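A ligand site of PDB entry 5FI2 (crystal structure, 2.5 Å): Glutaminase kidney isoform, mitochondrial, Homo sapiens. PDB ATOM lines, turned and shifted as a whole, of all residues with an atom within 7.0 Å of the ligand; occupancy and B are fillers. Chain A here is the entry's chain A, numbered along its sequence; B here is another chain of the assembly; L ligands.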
ATOM      1  N   ARG A 258      -4.023  31.080  -2.191  1.00  0.00           N
ATOM      2  CA  ARG A 258      -3.906  30.611  -0.812  1.00  0.00           C
ATOM      3  C   ARG A 258      -5.298  30.558  -0.174  1.00  0.00           C
ATOM      4  O   ARG A 258      -5.491  30.772   1.019  1.00  0.00           O
ATOM      5  CB  ARG A 258      -2.875  31.472  -0.035  1.00  0.00           C
ATOM      6  CG  ARG A 258      -2.713  31.404   1.520  1.00  0.00           C
ATOM      7  CD  ARG A 258      -3.005  30.071   2.232  1.00  0.00           C
ATOM      8  NE  ARG A 258      -2.745  28.913   1.402  1.00  0.00           N
ATOM      9  CZ  ARG A 258      -3.096  27.688   1.734  1.00  0.00           C
ATOM     10  NH1 ARG A 258      -3.732  27.458   2.881  1.00  0.00           N
ATOM     11  NH2 ARG A 258      -2.848  26.686   0.909  1.00  0.00           N
ATOM     12  N   PHE A 259      -6.288  30.291  -1.007  1.00  0.00           N
ATOM     13  CA  PHE A 259      -7.503  29.638  -0.562  1.00  0.00           C
ATOM     14  C   PHE A 259      -7.630  28.381  -1.417  1.00  0.00           C
ATOM     15  O   PHE A 259      -8.717  27.959  -1.829  1.00  0.00           O
ATOM     16  CB  PHE A 259      -8.722  30.567  -0.643  1.00  0.00           C
ATOM     17  CG  PHE A 259      -8.575  31.794   0.218  1.00  0.00           C
ATOM     18  CD1 PHE A 259      -8.772  31.725   1.596  1.00  0.00           C
ATOM     19  CD2 PHE A 259      -8.182  32.997  -0.328  1.00  0.00           C
ATOM     20  CE1 PHE A 259      -8.612  32.831   2.405  1.00  0.00           C
ATOM     21  CE2 PHE A 259      -8.022  34.105   0.472  1.00  0.00           C
ATOM     22  CZ  PHE A 259      -8.233  34.031   1.839  1.00  0.00           C
ATOM     23  N   LYS A 261      -7.154  25.295  -0.472  1.00  0.00           N
ATOM     24  CA  LYS A 261      -7.635  24.157   0.264  1.00  0.00           C
ATOM     25  C   LYS A 261      -9.108  24.264   0.518  1.00  0.00           C
ATOM     26  O   LYS A 261      -9.777  23.281   0.803  1.00  0.00           O
ATOM     27  CB  LYS A 261      -6.888  24.086   1.567  1.00  0.00           C
ATOM     28  CG  LYS A 261      -5.515  23.487   1.473  1.00  0.00           C
ATOM     29  CD  LYS A 261      -4.572  24.486   2.054  1.00  0.00           C
ATOM     30  CE  LYS A 261      -3.334  23.876   2.687  1.00  0.00           C
ATOM     31  NZ  LYS A 261      -3.742  23.178   3.924  1.00  0.00           N
ATOM     32  N   LEU A 262      -9.616  25.488   0.418  1.00  0.00           N
ATOM     33  CA  LEU A 262     -11.009  25.732   0.711  1.00  0.00           C
ATOM     34  C   LEU A 262     -11.858  25.261  -0.458  1.00  0.00           C
ATOM     35  O   LEU A 262     -11.523  25.494  -1.604  1.00  0.00           O
ATOM     36  CB  LEU A 262     -11.241  27.191   1.015  1.00  0.00           C
ATOM     37  CG  LEU A 262     -10.243  27.564   2.109  1.00  0.00           C
ATOM     38  CD1 LEU A 262     -10.349  29.015   2.397  1.00  0.00           C
ATOM     39  CD2 LEU A 262     -10.472  26.769   3.370  1.00  0.00           C
ATOM     40  N   PHE A 263     -12.926  24.569  -0.152  1.00  0.00           N
ATOM     41  CA  PHE A 263     -13.732  23.995  -1.201  1.00  0.00           C
ATOM     42  C   PHE A 263     -14.692  25.056  -1.712  1.00  0.00           C
ATOM     43  O   PHE A 263     -15.061  25.049  -2.885  1.00  0.00           O
ATOM     44  CB  PHE A 263     -14.482  22.767  -0.684  1.00  0.00           C
ATOM     45  CG  PHE A 263     -13.592  21.708  -0.110  1.00  0.00           C
ATOM     46  CD1 PHE A 263     -12.267  21.607  -0.498  1.00  0.00           C
ATOM     47  CD2 PHE A 263     -14.066  20.821   0.830  1.00  0.00           C
ATOM     48  CE1 PHE A 263     -11.453  20.636   0.036  1.00  0.00           C
ATOM     49  CE2 PHE A 263     -13.261  19.855   1.355  1.00  0.00           C
ATOM     50  CZ  PHE A 263     -11.945  19.759   0.958  1.00  0.00           C
ATOM     51  N   LEU A 264     -15.089  25.975  -0.839  1.00  0.00           N
ATOM     52  CA  LEU A 264     -16.158  26.894  -1.178  1.00  0.00           C
ATOM     53  C   LEU A 264     -15.769  28.336  -1.009  1.00  0.00           C
ATOM     54  O   LEU A 264     -14.994  28.676  -0.131  1.00  0.00           O
ATOM     55  CB  LEU A 264     -17.393  26.577  -0.349  1.00  0.00           C
ATOM     56  CG  LEU A 264     -17.964  25.166  -0.509  1.00  0.00           C
ATOM     57  CD1 LEU A 264     -19.171  24.964   0.370  1.00  0.00           C
ATOM     58  CD2 LEU A 264     -18.332  24.920  -1.956  1.00  0.00           C
ATOM     59  N   ASN A 265     -16.297  29.193  -1.876  1.00  0.00           N
ATOM     60  CA  ASN A 265     -16.142  30.610  -1.680  1.00  0.00           C
ATOM     61  C   ASN A 265     -17.170  31.038  -0.649  1.00  0.00           C
ATOM     62  O   ASN A 265     -17.850  30.208  -0.048  1.00  0.00           O
ATOM     63  CB  ASN A 265     -16.242  31.404  -3.000  1.00  0.00           C
ATOM     64  CG  ASN A 265     -17.617  31.357  -3.659  1.00  0.00           C
ATOM     65  OD1 ASN A 265     -18.628  31.146  -3.009  1.00  0.00           O
ATOM     66  ND2 ASN A 265     -17.634  31.552  -4.967  1.00  0.00           N
ATOM     67  N   GLU A 266     -17.288  32.337  -0.425  1.00  0.00           N
ATOM     68  CA  GLU A 266     -18.097  32.811   0.673  1.00  0.00           C
ATOM     69  C   GLU A 266     -19.593  32.720   0.386  1.00  0.00           C
ATOM     70  O   GLU A 266     -20.401  32.884   1.284  1.00  0.00           O
ATOM     71  CB  GLU A 266     -17.698  34.245   1.022  1.00  0.00           C
ATOM     72  CG  GLU A 266     -16.215  34.346   1.380  1.00  0.00           C
ATOM     73  CD  GLU A 266     -15.752  35.778   1.566  1.00  0.00           C
ATOM     74  OE1 GLU A 266     -16.446  36.526   2.293  1.00  0.00           O
ATOM     75  OE2 GLU A 266     -14.703  36.152   0.990  1.00  0.00           O
ATOM     76  N   ASP A 267     -19.951  32.432  -0.863  1.00  0.00           N
ATOM     77  CA  ASP A 267     -21.347  32.197  -1.207  1.00  0.00           C
ATOM     78  C   ASP A 267     -21.683  30.716  -1.161  1.00  0.00           C
ATOM     79  O   ASP A 267     -22.705  30.287  -1.686  1.00  0.00           O
ATOM     80  CB  ASP A 267     -21.665  32.760  -2.601  1.00  0.00           C
ATOM     81  CG  ASP A 267     -21.300  34.224  -2.740  1.00  0.00           C
ATOM     82  OD1 ASP A 267     -21.545  35.000  -1.806  1.00  0.00           O
ATOM     83  OD2 ASP A 267     -20.749  34.600  -3.790  1.00  0.00           O
ATOM     84  N   ASP A 268     -20.809  29.930  -0.531  1.00  0.00           N
ATOM     85  CA  ASP A 268     -20.944  28.484  -0.448  1.00  0.00           C
ATOM     86  C   ASP A 268     -21.005  27.802  -1.815  1.00  0.00           C
ATOM     87  O   ASP A 268     -21.709  26.816  -2.002  1.00  0.00           O
ATOM     88  CB  ASP A 268     -22.155  28.092   0.383  1.00  0.00           C
ATOM     89  CG  ASP A 268     -21.957  28.340   1.866  1.00  0.00           C
ATOM     90  OD1 ASP A 268     -20.803  28.495   2.301  1.00  0.00           O
ATOM     91  OD2 ASP A 268     -22.965  28.361   2.597  1.00  0.00           O
ATOM     92  N   HIS A 271     -15.010  27.720  -6.157  1.00  0.00           N
ATOM     93  CA  HIS A 271     -14.804  29.109  -6.579  1.00  0.00           C
ATOM     94  C   HIS A 271     -14.885  29.238  -8.102  1.00  0.00           C
ATOM     95  O   HIS A 271     -15.177  30.317  -8.595  1.00  0.00           O
ATOM     96  CB  HIS A 271     -13.491  29.759  -6.114  1.00  0.00           C
ATOM     97  CG  HIS A 271     -12.973  29.304  -4.798  1.00  0.00           C
ATOM     98  ND1 HIS A 271     -13.552  28.323  -4.034  1.00  0.00           N
ATOM     99  CD2 HIS A 271     -12.086  29.906  -3.970  1.00  0.00           C
ATOM    100  CE1 HIS A 271     -12.926  28.195  -2.892  1.00  0.00           C
ATOM    101  NE2 HIS A 271     -12.018  29.172  -2.825  1.00  0.00           N
ATOM    102  N   ARG A 328      -9.772  12.431  -0.981  1.00  0.00           N
ATOM    103  CA  ARG A 328     -10.000  13.862  -0.912  1.00  0.00           C
ATOM    104  C   ARG A 328     -11.185  14.241  -1.769  1.00  0.00           C
ATOM    105  O   ARG A 328     -11.965  15.105  -1.390  1.00  0.00           O
ATOM    106  CB  ARG A 328      -8.763  14.646  -1.346  1.00  0.00           C
ATOM    107  CG  ARG A 328      -9.101  16.052  -1.757  1.00  0.00           C
ATOM    108  CD  ARG A 328      -7.902  16.852  -2.198  1.00  0.00           C
ATOM    109  NE  ARG A 328      -7.652  17.945  -1.272  1.00  0.00           N
ATOM    110  CZ  ARG A 328      -8.100  19.192  -1.433  1.00  0.00           C
ATOM    111  NH1 ARG A 328      -8.811  19.502  -2.514  1.00  0.00           N
ATOM    112  NH2 ARG A 328      -7.824  20.114  -0.534  1.00  0.00           N
ATOM    113  N   TYR A 335     -18.556  17.159   1.788  1.00  0.00           N
ATOM    114  CA  TYR A 335     -18.641  18.578   2.103  1.00  0.00           C
ATOM    115  C   TYR A 335     -19.668  19.345   1.266  1.00  0.00           C
ATOM    116  O   TYR A 335     -20.437  20.127   1.808  1.00  0.00           O
ATOM    117  CB  TYR A 335     -17.271  19.242   1.945  1.00  0.00           C
ATOM    118  CG  TYR A 335     -17.139  20.563   2.655  1.00  0.00           C
ATOM    119  CD1 TYR A 335     -16.845  20.618   4.016  1.00  0.00           C
ATOM    120  CD2 TYR A 335     -17.324  21.753   1.977  1.00  0.00           C
ATOM    121  CE1 TYR A 335     -16.719  21.828   4.665  1.00  0.00           C
ATOM    122  CE2 TYR A 335     -17.208  22.965   2.637  1.00  0.00           C
ATOM    123  CZ  TYR A 335     -16.903  22.997   3.966  1.00  0.00           C
ATOM    124  OH  TYR A 335     -16.782  24.198   4.605  1.00  0.00           O
ATOM    125  N   LYS A 339     -23.200  21.017   2.411  1.00  0.00           N
ATOM    126  CA  LYS A 339     -23.431  22.442   2.169  1.00  0.00           C
ATOM    127  C   LYS A 339     -24.464  22.679   1.072  1.00  0.00           C
ATOM    128  O   LYS A 339     -24.686  23.809   0.671  1.00  0.00           O
ATOM    129  CB  LYS A 339     -22.122  23.126   1.803  1.00  0.00           C
ATOM    130  CG  LYS A 339     -21.185  23.279   2.979  1.00  0.00           C
ATOM    131  CD  LYS A 339     -21.757  24.283   3.957  1.00  0.00           C
ATOM    132  CE  LYS A 339     -20.809  24.575   5.105  1.00  0.00           C
ATOM    133  NZ  LYS A 339     -21.186  25.846   5.789  1.00  0.00           N
ATOM    134  N   ARG B 258     -11.670  37.444  -2.084  1.00  0.00           N
ATOM    135  CA  ARG B 258     -11.815  36.995  -0.694  1.00  0.00           C
ATOM    136  C   ARG B 258     -11.052  37.926   0.319  1.00  0.00           C
ATOM    137  O   ARG B 258     -11.316  39.135   0.370  1.00  0.00           O
ATOM    138  CB  ARG B 258     -11.363  35.539  -0.653  1.00  0.00           C
ATOM    139  CG  ARG B 258     -12.458  34.518  -0.979  1.00  0.00           C
ATOM    140  CD  ARG B 258     -11.901  33.104  -0.778  1.00  0.00           C
ATOM    141  NE  ARG B 258     -12.901  32.105  -0.503  1.00  0.00           N
ATOM    142  CZ  ARG B 258     -13.386  31.917   0.713  1.00  0.00           C
ATOM    143  NH1 ARG B 258     -13.006  32.702   1.717  1.00  0.00           N
ATOM    144  NH2 ARG B 258     -14.284  30.970   0.909  1.00  0.00           N
HETATM  145  C1  LIG L   1      -6.947  22.860   6.652  1.00  0.00           C
HETATM  146  C2  LIG L   1      -3.262  24.089   7.387  1.00  0.00           C
HETATM  147  C3  LIG L   1      -1.040  24.614   6.331  1.00  0.00           C
HETATM  148  C4  LIG L   1       0.220  22.981   5.090  1.00  0.00           C
HETATM  149  C5  LIG L   1     -13.670  25.269   3.698  1.00  0.00           C
HETATM  150  C6  LIG L   1     -13.677  29.783   3.501  1.00  0.00           C
HETATM  151  C7  LIG L   1     -12.157  21.785   4.026  1.00  0.00           C
HETATM  152  C8  LIG L   1     -12.641  22.923   3.083  1.00  0.00           C
HETATM  153  N1  LIG L   1     -12.863  24.134   4.007  1.00  0.00           N
HETATM  154  C9  LIG L   1     -12.541  23.725   5.203  1.00  0.00           C
HETATM  155  C10 LIG L   1     -11.592  22.423   4.969  1.00  0.00           C
HETATM  156  N2  LIG L   1     -10.309  22.824   4.478  1.00  0.00           N
HETATM  157  C11 LIG L   1      -9.188  22.760   5.386  1.00  0.00           C
HETATM  158  N3  LIG L   1      -9.188  22.316   6.652  1.00  0.00           N
HETATM  159  N4  LIG L   1      -8.007  22.365   7.317  1.00  0.00           N
HETATM  160  N5  LIG L   1      -5.612  23.019   7.181  1.00  0.00           N
HETATM  161  C12 LIG L   1      -4.641  23.979   6.723  1.00  0.00           C
HETATM  162  C13 LIG L   1      -2.038  23.683   6.562  1.00  0.00           C
HETATM  163  C14 LIG L   1       0.084  24.265   5.595  1.00  0.00           C
HETATM  164  C15 LIG L   1      -0.772  22.036   5.330  1.00  0.00           C
HETATM  165  C16 LIG L   1      -1.891  22.393   6.076  1.00  0.00           C
HETATM  166  O1  LIG L   1      -4.900  24.709   5.804  1.00  0.00           O
HETATM  167  S1  LIG L   1      -7.567  23.268   5.084  1.00  0.00           S
HETATM  168  N6  LIG L   1     -14.156  25.648   2.494  1.00  0.00           N
HETATM  169  N7  LIG L   1     -14.900  26.776   2.494  1.00  0.00           N
HETATM  170  C17 LIG L   1     -15.089  27.380   3.672  1.00  0.00           C
HETATM  171  N8  LIG L   1     -15.841  28.580   3.910  1.00  0.00           N
HETATM  172  C18 LIG L   1     -15.169  29.827   3.840  1.00  0.00           C
HETATM  173  C19 LIG L   1     -12.621  30.202   4.537  1.00  0.00           C
HETATM  174  C20 LIG L   1     -12.170  31.518   4.612  1.00  0.00           C
HETATM  175  C21 LIG L   1     -11.193  31.869   5.544  1.00  0.00           C
HETATM  176  C22 LIG L   1     -10.653  30.890   6.369  1.00  0.00           C
HETATM  177  C23 LIG L   1     -11.081  29.577   6.283  1.00  0.00           C
HETATM  178  C24 LIG L   1     -12.067  29.229   5.362  1.00  0.00           C
HETATM  179  O2  LIG L   1     -15.776  30.865   3.998  1.00  0.00           O
HETATM  180  S2  LIG L   1     -14.232  26.430   4.830  1.00  0.00           S
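An oxygen (O1) of the ligand lies within hydrogen-bond range of the side-chain amino group (NZ) of Lys 261 (2.7 Å).
NH2 of Arg 258 of chain B lies close to O2 of the ligand (3.4 Å).
The backbone NH (N) of Phe 263 is in hydrogen-bond range of a nitrogen (N6) of the ligand, at 3.1 Å.
N of Leu 264 sits at hydrogen-bond distance from N7 of the ligand (3.4 Å).
The side-chain hydroxyl (OH) of Tyr 335 lies close to a sulfur (S2) of the ligand, 3.4 Å away.
NH2 of Arg 258 of chain B is in hydrogen-bond range of O of Leu 264, 2.6 Å away.
NH1 of Arg 258 of chain B is in salt-bridge range of OE2 of Glu 266 (3.9 Å).
Residues that only touch the ligand: Leu 262.
Hydrophobic or aromatic side chains within 4 Å of the ligand: Leu 262, Phe 263, Leu 264 and Tyr 335.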
